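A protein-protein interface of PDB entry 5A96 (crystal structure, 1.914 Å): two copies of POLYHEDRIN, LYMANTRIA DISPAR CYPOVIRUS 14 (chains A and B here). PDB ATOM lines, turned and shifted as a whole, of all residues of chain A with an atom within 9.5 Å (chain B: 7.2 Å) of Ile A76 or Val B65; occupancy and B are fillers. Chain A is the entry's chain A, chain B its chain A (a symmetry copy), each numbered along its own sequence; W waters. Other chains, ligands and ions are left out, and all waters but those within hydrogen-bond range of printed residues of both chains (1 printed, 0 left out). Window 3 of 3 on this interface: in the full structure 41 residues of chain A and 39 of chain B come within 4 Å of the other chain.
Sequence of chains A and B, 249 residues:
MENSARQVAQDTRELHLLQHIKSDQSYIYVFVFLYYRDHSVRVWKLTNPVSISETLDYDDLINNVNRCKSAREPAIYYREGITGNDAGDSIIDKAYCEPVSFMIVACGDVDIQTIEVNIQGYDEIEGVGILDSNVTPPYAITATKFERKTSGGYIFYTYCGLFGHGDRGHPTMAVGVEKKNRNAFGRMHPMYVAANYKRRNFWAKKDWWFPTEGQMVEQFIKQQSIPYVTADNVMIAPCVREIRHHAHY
OE1 of Glu A80 sits close to O of Trp B209, at 2.7 Å.
OG1 of Thr A83 lies within hydrogen-bond range of O of Arg A79 (2.8 Å). The indole nitrogen of Trp B209 lies within hydrogen-bond range of the side-chain hydroxyl of Ser B40. The backbone NH of Val B41 is in hydrogen-bond range of the backbone carbonyl oxygen of Phe B210 (2.9 Å). N of Val B65 lies within hydrogen-bond range of OD1 of Asn B63 (3.0 Å). NE1 of Trp B209 is in hydrogen-bond range of OD1 of Asn B63. SG of Cys B97 is disulfide-bonded to SG of Cys B68.
Ile A76 touches Val B65 (CG2 to CG1, 3.8 Å). Trp B209 touches Ile A76 (CE3 to CG1, 3.5 Å). Glu A80 touches Phe B210 (OE2 to CD1, 3.3 Å). CD of Pro B211 touches OE2 of Glu A80 (3.6 Å). Thr A83 touches Trp B208 (CG2 to CD1, 3.4 Å). Thr A83 touches Phe B210. Tyr A122 touches Trp B208 (CE2 to CD1, 3.8 Å).
Printed residues of chain B within 4 Å of Ile A76: Val B65 and Trp B209. Val B65 touches one residue of chain A. Asn B64 touches none of the printed residues of chain A. Trp B209 touches just these residues of chain A: Ile A76 (3.5 Å) and Glu A80 (2.7 Å). Of the printed residues of chain B, Glu A80 touches Trp B209, Phe B210 and Pro B211. Of the printed residues of chain A, Trp B208 touches Thr A83 (3.4 Å) and Tyr A122 (3.8 Å). Of the printed residues of chain A, Phe B210 touches Glu A80 (3.3 Å) and Thr A83 (3.7 Å). Printed residues of chain A within 4 Å of Pro B211: Glu A80 (3.6 Å). The nearest residue of chain A that does not touch Val B65 is Pro A74 (6.6 Å).
Printed residues of chain B that touch a printed residue of chain A: Val B65, Trp B208, Trp B209, Phe B210 and Pro B211. Hydrophobic or aromatic side chains of chain A within 4 Å of the printed part of chain B: Ile A76 and Tyr A122. Along chain A the printed residues that touch a printed residue of chain B span positions 76 to 122.
Position printed for both chains: 68. Of the 8 pairs that touch across the chains among the printed residues, none has its exchanged pair printed and touching as well.
Water W1 lies within hydrogen-bond range of OG1 of Thr A83 (2.8 Å), N of Trp B209 (3.2 Å) and OE1 of Glu A80 (3.5 Å).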
ATOM      1  N   TYR A  58      26.596 -12.406 -31.325  1.00  0.00           N
ATOM      2  CA  TYR A  58      26.070 -12.839 -30.036  1.00  0.00           C
ATOM      3  C   TYR A  58      24.721 -13.552 -30.162  1.00  0.00           C
ATOM      4  O   TYR A  58      24.504 -14.611 -29.559  1.00  0.00           O
ATOM      5  CB  TYR A  58      25.947 -11.625 -29.112  1.00  0.00           C
ATOM      6  CG  TYR A  58      25.476 -11.954 -27.715  1.00  0.00           C
ATOM      7  CD1 TYR A  58      26.347 -12.502 -26.772  1.00  0.00           C
ATOM      8  CD2 TYR A  58      24.157 -11.713 -27.331  1.00  0.00           C
ATOM      9  CE1 TYR A  58      25.914 -12.810 -25.483  1.00  0.00           C
ATOM     10  CE2 TYR A  58      23.724 -12.002 -26.050  1.00  0.00           C
ATOM     11  CZ  TYR A  58      24.610 -12.553 -25.131  1.00  0.00           C
ATOM     12  OH  TYR A  58      24.177 -12.841 -23.855  1.00  0.00           O
ATOM     13  N   CYS A  68      16.562 -17.108 -22.679  1.00  0.00           N
ATOM     14  CA  CYS A  68      16.613 -16.333 -21.451  1.00  0.00           C
ATOM     15  C   CYS A  68      15.616 -15.190 -21.567  1.00  0.00           C
ATOM     16  O   CYS A  68      15.810 -14.264 -22.355  1.00  0.00           O
ATOM     17  CB  CYS A  68      18.019 -15.784 -21.234  1.00  0.00           C
ATOM     18  SG  CYS A  68      19.314 -16.989 -21.541  1.00  0.00           S
ATOM     19  N   GLU A  73      12.657  -7.917 -17.241  1.00  0.00           N
ATOM     20  CA  GLU A  73      13.681  -7.039 -17.797  1.00  0.00           C
ATOM     21  C   GLU A  73      13.836  -7.253 -19.313  1.00  0.00           C
ATOM     22  O   GLU A  73      14.108  -8.367 -19.759  1.00  0.00           O
ATOM     23  CB  GLU A  73      15.023  -7.234 -17.058  1.00  0.00           C
ATOM     24  CG  GLU A  73      14.972  -6.821 -15.566  1.00  0.00           C
ATOM     25  CD  GLU A  73      16.348  -6.715 -14.882  1.00  0.00           C
ATOM     26  OE1 GLU A  73      17.222  -7.583 -15.092  1.00  0.00           O
ATOM     27  OE2 GLU A  73      16.547  -5.756 -14.106  1.00  0.00           O
ATOM     28  N   PRO A  74      13.640  -6.181 -20.111  1.00  0.00           N
ATOM     29  CA  PRO A  74      13.898  -6.220 -21.561  1.00  0.00           C
ATOM     30  C   PRO A  74      15.352  -6.573 -21.876  1.00  0.00           C
ATOM     31  O   PRO A  74      16.211  -6.441 -21.000  1.00  0.00           O
ATOM     32  CB  PRO A  74      13.609  -4.785 -22.015  1.00  0.00           C
ATOM     33  CG  PRO A  74      13.648  -3.960 -20.774  1.00  0.00           C
ATOM     34  CD  PRO A  74      13.182  -4.850 -19.673  1.00  0.00           C
ATOM     35  N   ALA A  75      15.624  -6.984 -23.110  1.00  0.00           N
ATOM     36  CA  ALA A  75      16.940  -7.510 -23.473  1.00  0.00           C
ATOM     37  C   ALA A  75      18.038  -6.460 -23.308  1.00  0.00           C
ATOM     38  O   ALA A  75      19.148  -6.777 -22.879  1.00  0.00           O
ATOM     39  CB  ALA A  75      16.922  -8.054 -24.901  1.00  0.00           C
ATOM     40  N   ILE A  76      17.724  -5.209 -23.628  1.00  0.00           N
ATOM     41  CA  ILE A  76      18.707  -4.134 -23.540  1.00  0.00           C
ATOM     42  C   ILE A  76      19.250  -3.907 -22.112  1.00  0.00           C
ATOM     43  O   ILE A  76      20.354  -3.394 -21.959  1.00  0.00           O
ATOM     44  CB  ILE A  76      18.139  -2.809 -24.089  1.00  0.00           C
ATOM     45  CG1 ILE A  76      19.264  -1.777 -24.288  1.00  0.00           C
ATOM     46  CG2 ILE A  76      17.050  -2.250 -23.160  1.00  0.00           C
ATOM     47  CD1 ILE A  76      20.268  -2.152 -25.385  1.00  0.00           C
ATOM     48  N   TYR A  77      18.487  -4.265 -21.071  1.00  0.00           N
ATOM     49  CA  TYR A  77      18.978  -4.096 -19.687  1.00  0.00           C
ATOM     50  C   TYR A  77      20.270  -4.883 -19.469  1.00  0.00           C
ATOM     51  O   TYR A  77      21.192  -4.421 -18.790  1.00  0.00           O
ATOM     52  CB  TYR A  77      17.944  -4.569 -18.663  1.00  0.00           C
ATOM     53  CG  TYR A  77      16.826  -3.592 -18.436  1.00  0.00           C
ATOM     54  CD1 TYR A  77      16.460  -2.690 -19.423  1.00  0.00           C
ATOM     55  CD2 TYR A  77      16.132  -3.566 -17.233  1.00  0.00           C
ATOM     56  CE1 TYR A  77      15.436  -1.787 -19.227  1.00  0.00           C
ATOM     57  CE2 TYR A  77      15.099  -2.658 -17.024  1.00  0.00           C
ATOM     58  CZ  TYR A  77      14.759  -1.773 -18.034  1.00  0.00           C
ATOM     59  OH  TYR A  77      13.740  -0.867 -17.860  1.00  0.00           O
ATOM     60  N   TYR A  78      20.306  -6.083 -20.047  1.00  0.00           N
ATOM     61  CA  TYR A  78      21.467  -6.943 -20.001  1.00  0.00           C
ATOM     62  C   TYR A  78      22.495  -6.573 -21.061  1.00  0.00           C
ATOM     63  O   TYR A  78      23.681  -6.490 -20.750  1.00  0.00           O
ATOM     64  CB  TYR A  78      21.034  -8.393 -20.212  1.00  0.00           C
ATOM     65  CG  TYR A  78      22.176  -9.387 -20.147  1.00  0.00           C
ATOM     66  CD1 TYR A  78      22.620  -9.878 -18.928  1.00  0.00           C
ATOM     67  CD2 TYR A  78      22.792  -9.850 -21.305  1.00  0.00           C
ATOM     68  CE1 TYR A  78      23.653 -10.802 -18.863  1.00  0.00           C
ATOM     69  CE2 TYR A  78      23.833 -10.764 -21.248  1.00  0.00           C
ATOM     70  CZ  TYR A  78      24.252 -11.241 -20.023  1.00  0.00           C
ATOM     71  OH  TYR A  78      25.279 -12.153 -19.951  1.00  0.00           O
ATOM     72  N   ARG A  79      22.048  -6.351 -22.304  1.00  0.00           N
ATOM     73  CA  ARG A  79      22.960  -6.041 -23.417  1.00  0.00           C
ATOM     74  C   ARG A  79      23.814  -4.824 -23.125  1.00  0.00           C
ATOM     75  O   ARG A  79      24.989  -4.800 -23.476  1.00  0.00           O
ATOM     76  CB  ARG A  79      22.214  -5.758 -24.721  1.00  0.00           C
ATOM     77  CG  ARG A  79      21.392  -6.887 -25.261  1.00  0.00           C
ATOM     78  CD  ARG A  79      22.214  -8.107 -25.526  1.00  0.00           C
ATOM     79  NE  ARG A  79      21.364  -9.239 -25.910  1.00  0.00           N
ATOM     80  CZ  ARG A  79      21.134  -9.632 -27.161  1.00  0.00           C
ATOM     81  NH1 ARG A  79      21.684  -8.995 -28.189  1.00  0.00           N
ATOM     82  NH2 ARG A  79      20.350 -10.677 -27.386  1.00  0.00           N
ATOM     83  N   GLU A  80      23.224  -3.803 -22.509  1.00  0.00           N
ATOM     84  CA  GLU A  80      23.979  -2.592 -22.201  1.00  0.00           C
ATOM     85  C   GLU A  80      25.150  -2.893 -21.262  1.00  0.00           C
ATOM     86  O   GLU A  80      26.197  -2.243 -21.331  1.00  0.00           O
ATOM     87  CB  GLU A  80      23.076  -1.527 -21.583  1.00  0.00           C
ATOM     88  CG  GLU A  80      23.642  -0.121 -21.674  1.00  0.00           C
ATOM     89  CD  GLU A  80      23.494   0.502 -23.063  1.00  0.00           C
ATOM     90  OE1 GLU A  80      23.003  -0.184 -23.990  1.00  0.00           O
ATOM     91  OE2 GLU A  80      23.865   1.691 -23.209  1.00  0.00           O
ATOM     92  N   GLY A  81      24.974  -3.875 -20.381  1.00  0.00           N
ATOM     93  CA  GLY A  81      26.007  -4.230 -19.430  1.00  0.00           C
ATOM     94  C   GLY A  81      27.158  -5.019 -20.043  1.00  0.00           C
ATOM     95  O   GLY A  81      28.257  -5.046 -19.487  1.00  0.00           O
ATOM     96  N   ILE A  82      26.923  -5.673 -21.179  1.00  0.00           N
ATOM     97  CA  ILE A  82      28.026  -6.317 -21.892  1.00  0.00           C
ATOM     98  C   ILE A  82      28.458  -5.470 -23.104  1.00  0.00           C
ATOM     99  O   ILE A  82      29.342  -5.862 -23.863  1.00  0.00           O
ATOM    100  CB  ILE A  82      27.682  -7.771 -22.306  1.00  0.00           C
ATOM    101  CG1 ILE A  82      26.450  -7.807 -23.220  1.00  0.00           C
ATOM    102  CG2 ILE A  82      27.415  -8.633 -21.054  1.00  0.00           C
ATOM    103  CD1 ILE A  82      26.154  -9.197 -23.813  1.00  0.00           C
ATOM    104  N   THR A  83      27.830  -4.306 -23.273  1.00  0.00           N
ATOM    105  CA  THR A  83      28.263  -3.330 -24.279  1.00  0.00           C
ATOM    106  C   THR A  83      29.350  -2.409 -23.720  1.00  0.00           C
ATOM    107  O   THR A  83      30.348  -2.121 -24.371  1.00  0.00           O
ATOM    108  CB  THR A  83      27.097  -2.438 -24.741  1.00  0.00           C
ATOM    109  OG1 THR A  83      26.136  -3.228 -25.453  1.00  0.00           O
ATOM    110  CG2 THR A  83      27.610  -1.304 -25.647  1.00  0.00           C
ATOM    111  N   GLY A  84      29.144  -1.924 -22.506  1.00  0.00           N
ATOM    112  CA  GLY A  84      30.128  -1.068 -21.881  1.00  0.00           C
ATOM    113  C   GLY A  84      30.340  -1.469 -20.440  1.00  0.00           C
ATOM    114  O   GLY A  84      29.452  -2.047 -19.810  1.00  0.00           O
ATOM    115  N   ALA A  87      27.901  -0.601 -17.425  1.00  0.00           N
ATOM    116  CA  ALA A  87      26.809   0.165 -18.030  1.00  0.00           C
ATOM    117  C   ALA A  87      25.468  -0.604 -18.044  1.00  0.00           C
ATOM    118  O   ALA A  87      24.527  -0.194 -18.723  1.00  0.00           O
ATOM    119  CB  ALA A  87      27.180   0.579 -19.451  1.00  0.00           C
ATOM    120  N   GLY A  88      25.379  -1.697 -17.291  1.00  0.00           N
ATOM    121  CA  GLY A  88      24.185  -2.533 -17.289  1.00  0.00           C
ATOM    122  C   GLY A  88      23.100  -2.074 -16.328  1.00  0.00           C
ATOM    123  O   GLY A  88      23.343  -1.281 -15.417  1.00  0.00           O
ATOM    124  N   ASP A  89      21.888  -2.578 -16.532  1.00  0.00           N
ATOM    125  CA  ASP A  89      20.782  -2.301 -15.625  1.00  0.00           C
ATOM    126  C   ASP A  89      20.002  -3.590 -15.467  1.00  0.00           C
ATOM    127  O   ASP A  89      18.781  -3.641 -15.636  1.00  0.00           O
ATOM    128  CB  ASP A  89      19.894  -1.180 -16.168  1.00  0.00           C
ATOM    129  CG  ASP A  89      18.858  -0.710 -15.163  1.00  0.00           C
ATOM    130  OD1 ASP A  89      18.987  -1.029 -13.964  1.00  0.00           O
ATOM    131  OD2 ASP A  89      17.902  -0.026 -15.576  1.00  0.00           O
ATOM    132  N   SER A  90      20.743  -4.635 -15.140  1.00  0.00           N
ATOM    133  CA  SER A  90      20.218  -5.990 -15.074  1.00  0.00           C
ATOM    134  C   SER A  90      20.554  -6.591 -13.715  1.00  0.00           C
ATOM    135  O   SER A  90      21.668  -6.408 -13.218  1.00  0.00           O
ATOM    136  CB  SER A  90      20.862  -6.822 -16.185  1.00  0.00           C
ATOM    137  OG  SER A  90      20.510  -8.191 -16.108  1.00  0.00           O
ATOM    138  N   TYR A 122      31.284  -9.057 -26.696  1.00  0.00           N
ATOM    139  CA  TYR A 122      30.066  -8.620 -27.342  1.00  0.00           C
ATOM    140  C   TYR A 122      30.334  -7.586 -28.427  1.00  0.00           C
ATOM    141  O   TYR A 122      29.663  -7.568 -29.455  1.00  0.00           O
ATOM    142  CB  TYR A 122      29.133  -8.020 -26.288  1.00  0.00           C
ATOM    143  CG  TYR A 122      27.743  -7.706 -26.784  1.00  0.00           C
ATOM    144  CD1 TYR A 122      26.822  -8.720 -27.045  1.00  0.00           C
ATOM    145  CD2 TYR A 122      27.338  -6.391 -26.977  1.00  0.00           C
ATOM    146  CE1 TYR A 122      25.531  -8.425 -27.494  1.00  0.00           C
ATOM    147  CE2 TYR A 122      26.056  -6.088 -27.419  1.00  0.00           C
ATOM    148  CZ  TYR A 122      25.159  -7.107 -27.676  1.00  0.00           C
ATOM    149  OH  TYR A 122      23.897  -6.791 -28.116  1.00  0.00           O
ATOM    150  N   TYR B  36      17.424   9.212 -32.652  1.00  0.00           N
ATOM    151  CA  TYR B  36      15.961   9.203 -32.638  1.00  0.00           C
ATOM    152  C   TYR B  36      15.391  10.381 -31.836  1.00  0.00           C
ATOM    153  O   TYR B  36      16.115  11.080 -31.125  1.00  0.00           O
ATOM    154  CB  TYR B  36      15.460   7.855 -32.100  1.00  0.00           C
ATOM    155  CG  TYR B  36      16.083   6.704 -32.862  1.00  0.00           C
ATOM    156  CD1 TYR B  36      15.588   6.327 -34.104  1.00  0.00           C
ATOM    157  CD2 TYR B  36      17.188   6.025 -32.364  1.00  0.00           C
ATOM    158  CE1 TYR B  36      16.160   5.298 -34.826  1.00  0.00           C
ATOM    159  CE2 TYR B  36      17.770   4.971 -33.076  1.00  0.00           C
ATOM    160  CZ  TYR B  36      17.252   4.629 -34.313  1.00  0.00           C
ATOM    161  OH  TYR B  36      17.815   3.611 -35.041  1.00  0.00           O
ATOM    162  N   ASP B  38      13.587  10.365 -29.297  1.00  0.00           N
ATOM    163  CA  ASP B  38      13.644  10.116 -27.855  1.00  0.00           C
ATOM    164  C   ASP B  38      15.045  10.328 -27.282  1.00  0.00           C
ATOM    165  O   ASP B  38      15.301  10.004 -26.115  1.00  0.00           O
ATOM    166  CB  ASP B  38      13.139   8.697 -27.511  1.00  0.00           C
ATOM    167  CG  ASP B  38      14.020   7.589 -28.081  1.00  0.00           C
ATOM    168  OD1 ASP B  38      15.006   7.900 -28.781  1.00  0.00           O
ATOM    169  OD2 ASP B  38      13.718   6.398 -27.840  1.00  0.00           O
ATOM    170  N   SER B  40      17.709   8.750 -27.964  1.00  0.00           N
ATOM    171  CA  SER B  40      18.531   7.538 -27.969  1.00  0.00           C
ATOM    172  C   SER B  40      19.331   7.432 -29.271  1.00  0.00           C
ATOM    173  O   SER B  40      19.043   8.123 -30.240  1.00  0.00           O
ATOM    174  CB  SER B  40      17.664   6.282 -27.761  1.00  0.00           C
ATOM    175  OG  SER B  40      16.884   5.961 -28.908  1.00  0.00           O
ATOM    176  N   VAL B  41      20.343   6.568 -29.281  1.00  0.00           N
ATOM    177  CA  VAL B  41      21.188   6.385 -30.450  1.00  0.00           C
ATOM    178  C   VAL B  41      21.320   4.900 -30.756  1.00  0.00           C
ATOM    179  O   VAL B  41      21.626   4.107 -29.870  1.00  0.00           O
ATOM    180  CB  VAL B  41      22.604   6.964 -30.202  1.00  0.00           C
ATOM    181  CG1 VAL B  41      23.407   7.022 -31.498  1.00  0.00           C
ATOM    182  CG2 VAL B  41      22.500   8.342 -29.593  1.00  0.00           C
ATOM    183  N   ARG B  42      21.082   4.519 -32.002  1.00  0.00           N
ATOM    184  CA  ARG B  42      21.444   3.180 -32.447  1.00  0.00           C
ATOM    185  C   ARG B  42      22.684   3.314 -33.299  1.00  0.00           C
ATOM    186  O   ARG B  42      22.789   4.236 -34.104  1.00  0.00           O
ATOM    187  CB  ARG B  42      20.325   2.513 -33.236  1.00  0.00           C
ATOM    188  CG  ARG B  42      20.615   1.055 -33.580  1.00  0.00           C
ATOM    189  CD  ARG B  42      19.367   0.372 -34.107  1.00  0.00           C
ATOM    190  NE  ARG B  42      19.586  -1.054 -34.360  1.00  0.00           N
ATOM    191  CZ  ARG B  42      18.698  -1.872 -34.919  1.00  0.00           C
ATOM    192  NH1 ARG B  42      17.517  -1.415 -35.314  1.00  0.00           N
ATOM    193  NH2 ARG B  42      18.996  -3.160 -35.095  1.00  0.00           N
ATOM    194  N   ILE B  62      15.710   1.680 -37.917  1.00  0.00           N
ATOM    195  CA  ILE B  62      14.741   2.154 -36.924  1.00  0.00           C
ATOM    196  C   ILE B  62      15.164   1.771 -35.509  1.00  0.00           C
ATOM    197  O   ILE B  62      15.970   0.874 -35.316  1.00  0.00           O
ATOM    198  CB  ILE B  62      13.329   1.588 -37.179  1.00  0.00           C
ATOM    199  CG1 ILE B  62      13.318   0.061 -36.985  1.00  0.00           C
ATOM    200  CG2 ILE B  62      12.865   1.983 -38.556  1.00  0.00           C
ATOM    201  CD1 ILE B  62      11.943  -0.564 -37.160  1.00  0.00           C
ATOM    202  N   ASN B  63      14.606   2.468 -34.532  1.00  0.00           N
ATOM    203  CA  ASN B  63      14.886   2.231 -33.126  1.00  0.00           C
ATOM    204  C   ASN B  63      14.250   0.914 -32.694  1.00  0.00           C
ATOM    205  O   ASN B  63      13.028   0.782 -32.684  1.00  0.00           O
ATOM    206  CB  ASN B  63      14.330   3.399 -32.289  1.00  0.00           C
ATOM    207  CG  ASN B  63      14.721   3.311 -30.810  1.00  0.00           C
ATOM    208  OD1 ASN B  63      15.110   2.257 -30.319  1.00  0.00           O
ATOM    209  ND2 ASN B  63      14.615   4.426 -30.103  1.00  0.00           N
ATOM    210  N   ASN B  64      15.070  -0.075 -32.354  1.00  0.00           N
ATOM    211  CA  ASN B  64      14.524  -1.372 -31.982  1.00  0.00           C
ATOM    212  C   ASN B  64      14.539  -1.636 -30.485  1.00  0.00           C
ATOM    213  O   ASN B  64      14.306  -2.764 -30.069  1.00  0.00           O
ATOM    214  CB  ASN B  64      15.259  -2.502 -32.704  1.00  0.00           C
ATOM    215  CG  ASN B  64      16.680  -2.665 -32.232  1.00  0.00           C
ATOM    216  OD1 ASN B  64      17.286  -1.728 -31.710  1.00  0.00           O
ATOM    217  ND2 ASN B  64      17.234  -3.854 -32.431  1.00  0.00           N
ATOM    218  N   VAL B  65      14.811  -0.609 -29.681  1.00  0.00           N
ATOM    219  CA  VAL B  65      14.715  -0.734 -28.225  1.00  0.00           C
ATOM    220  C   VAL B  65      13.465  -0.006 -27.704  1.00  0.00           C
ATOM    221  O   VAL B  65      12.644  -0.577 -26.983  1.00  0.00           O
ATOM    222  CB  VAL B  65      15.978  -0.199 -27.543  1.00  0.00           C
ATOM    223  CG1 VAL B  65      15.775  -0.092 -26.047  1.00  0.00           C
ATOM    224  CG2 VAL B  65      17.172  -1.104 -27.862  1.00  0.00           C
ATOM    225  N   ASN B  66      13.322   1.262 -28.068  1.00  0.00           N
ATOM    226  CA  ASN B  66      12.081   1.968 -27.813  1.00  0.00           C
ATOM    227  C   ASN B  66      11.207   1.747 -29.058  1.00  0.00           C
ATOM    228  O   ASN B  66      11.187   2.562 -29.988  1.00  0.00           O
ATOM    229  CB  ASN B  66      12.345   3.449 -27.520  1.00  0.00           C
ATOM    230  CG  ASN B  66      11.091   4.188 -27.057  1.00  0.00           C
ATOM    231  OD1 ASN B  66      10.046   3.578 -26.821  1.00  0.00           O
ATOM    232  ND2 ASN B  66      11.189   5.508 -26.931  1.00  0.00           N
ATOM    233  N   ARG B  67      10.509   0.613 -29.074  1.00  0.00           N
ATOM    234  CA  ARG B  67       9.915   0.095 -30.303  1.00  0.00           C
ATOM    235  C   ARG B  67       8.520   0.639 -30.586  1.00  0.00           C
ATOM    236  O   ARG B  67       7.760   0.951 -29.674  1.00  0.00           O
ATOM    237  CB  ARG B  67       9.863  -1.436 -30.264  1.00  0.00           C
ATOM    238  CG  ARG B  67      11.157  -2.102 -30.694  1.00  0.00           C
ATOM    239  CD  ARG B  67      10.959  -3.591 -30.909  1.00  0.00           C
ATOM    240  NE  ARG B  67      10.526  -4.255 -29.683  1.00  0.00           N
ATOM    241  CZ  ARG B  67      11.345  -4.844 -28.817  1.00  0.00           C
ATOM    242  NH1 ARG B  67      12.654  -4.870 -29.035  1.00  0.00           N
ATOM    243  NH2 ARG B  67      10.854  -5.415 -27.729  1.00  0.00           N
ATOM    244  N   CYS B  68       8.189   0.745 -31.865  1.00  0.00           N
ATOM    245  CA  CYS B  68       6.857   1.169 -32.261  1.00  0.00           C
ATOM    246  C   CYS B  68       5.966  -0.060 -32.331  1.00  0.00           C
ATOM    247  O   CYS B  68       6.135  -0.910 -33.205  1.00  0.00           O
ATOM    248  CB  CYS B  68       6.908   1.860 -33.620  1.00  0.00           C
ATOM    249  SG  CYS B  68       8.263   3.028 -33.780  1.00  0.00           S
ATOM    250  N   CYS B  97       9.731   5.578 -34.501  1.00  0.00           N
ATOM    251  CA  CYS B  97      11.023   4.910 -34.325  1.00  0.00           C
ATOM    252  C   CYS B  97      11.969   5.092 -35.515  1.00  0.00           C
ATOM    253  O   CYS B  97      13.055   4.524 -35.544  1.00  0.00           O
ATOM    254  CB  CYS B  97      10.812   3.414 -34.031  1.00  0.00           C
ATOM    255  SG  CYS B  97       9.705   2.580 -35.182  1.00  0.00           S
ATOM    256  N   TRP B 208      24.559  -1.572 -31.586  1.00  0.00           N
ATOM    257  CA  TRP B 208      24.283  -1.359 -30.169  1.00  0.00           C
ATOM    258  C   TRP B 208      23.232  -0.272 -30.076  1.00  0.00           C
ATOM    259  O   TRP B 208      22.920   0.380 -31.070  1.00  0.00           O
ATOM    260  CB  TRP B 208      25.524  -0.855 -29.430  1.00  0.00           C
ATOM    261  CG  TRP B 208      26.762  -1.707 -29.571  1.00  0.00           C
ATOM    262  CD1 TRP B 208      27.177  -2.686 -28.724  1.00  0.00           C
ATOM    263  CD2 TRP B 208      27.745  -1.636 -30.616  1.00  0.00           C
ATOM    264  NE1 TRP B 208      28.355  -3.227 -29.164  1.00  0.00           N
ATOM    265  CE2 TRP B 208      28.726  -2.605 -30.328  1.00  0.00           C
ATOM    266  CE3 TRP B 208      27.890  -0.848 -31.762  1.00  0.00           C
ATOM    267  CZ2 TRP B 208      29.843  -2.807 -31.142  1.00  0.00           C
ATOM    268  CZ3 TRP B 208      28.991  -1.048 -32.575  1.00  0.00           C
ATOM    269  CH2 TRP B 208      29.959  -2.022 -32.259  1.00  0.00           C
ATOM    270  N   TRP B 209      22.701  -0.056 -28.880  1.00  0.00           N
ATOM    271  CA  TRP B 209      21.786   1.063 -28.638  1.00  0.00           C
ATOM    272  C   TRP B 209      22.159   1.699 -27.311  1.00  0.00           C
ATOM    273  O   TRP B 209      22.647   1.014 -26.408  1.00  0.00           O
ATOM    274  CB  TRP B 209      20.344   0.554 -28.617  1.00  0.00           C
ATOM    275  CG  TRP B 209      19.297   1.566 -28.225  1.00  0.00           C
ATOM    276  CD1 TRP B 209      18.515   2.313 -29.065  1.00  0.00           C
ATOM    277  CD2 TRP B 209      18.896   1.913 -26.890  1.00  0.00           C
ATOM    278  NE1 TRP B 209      17.661   3.116 -28.332  1.00  0.00           N
ATOM    279  CE2 TRP B 209      17.877   2.889 -26.996  1.00  0.00           C
ATOM    280  CE3 TRP B 209      19.301   1.502 -25.620  1.00  0.00           C
ATOM    281  CZ2 TRP B 209      17.260   3.450 -25.875  1.00  0.00           C
ATOM    282  CZ3 TRP B 209      18.697   2.077 -24.509  1.00  0.00           C
ATOM    283  CH2 TRP B 209      17.686   3.032 -24.647  1.00  0.00           C
ATOM    284  N   PHE B 210      21.938   3.008 -27.212  1.00  0.00           N
ATOM    285  CA  PHE B 210      22.301   3.786 -26.040  1.00  0.00           C
ATOM    286  C   PHE B 210      21.194   4.794 -25.758  1.00  0.00           C
ATOM    287  O   PHE B 210      20.606   5.333 -26.693  1.00  0.00           O
ATOM    288  CB  PHE B 210      23.611   4.524 -26.296  1.00  0.00           C
ATOM    289  CG  PHE B 210      24.733   3.619 -26.714  1.00  0.00           C
ATOM    290  CD1 PHE B 210      25.550   3.035 -25.768  1.00  0.00           C
ATOM    291  CD2 PHE B 210      24.953   3.332 -28.052  1.00  0.00           C
ATOM    292  CE1 PHE B 210      26.580   2.189 -26.148  1.00  0.00           C
ATOM    293  CE2 PHE B 210      25.992   2.480 -28.435  1.00  0.00           C
ATOM    294  CZ  PHE B 210      26.794   1.916 -27.483  1.00  0.00           C
ATOM    295  N   PRO B 211      20.895   5.041 -24.469  1.00  0.00           N
ATOM    296  CA  PRO B 211      19.785   5.931 -24.080  1.00  0.00           C
ATOM    297  C   PRO B 211      20.009   7.415 -24.463  1.00  0.00           C
ATOM    298  O   PRO B 211      19.043   8.121 -24.769  1.00  0.00           O
ATOM    299  CB  PRO B 211      19.691   5.745 -22.557  1.00  0.00           C
ATOM    300  CG  PRO B 211      21.005   5.160 -22.136  1.00  0.00           C
ATOM    301  CD  PRO B 211      21.559   4.419 -23.311  1.00  0.00           C
HETATM  302  O   HOH W   1      23.896  -2.133 -26.749  1.00  0.00           O
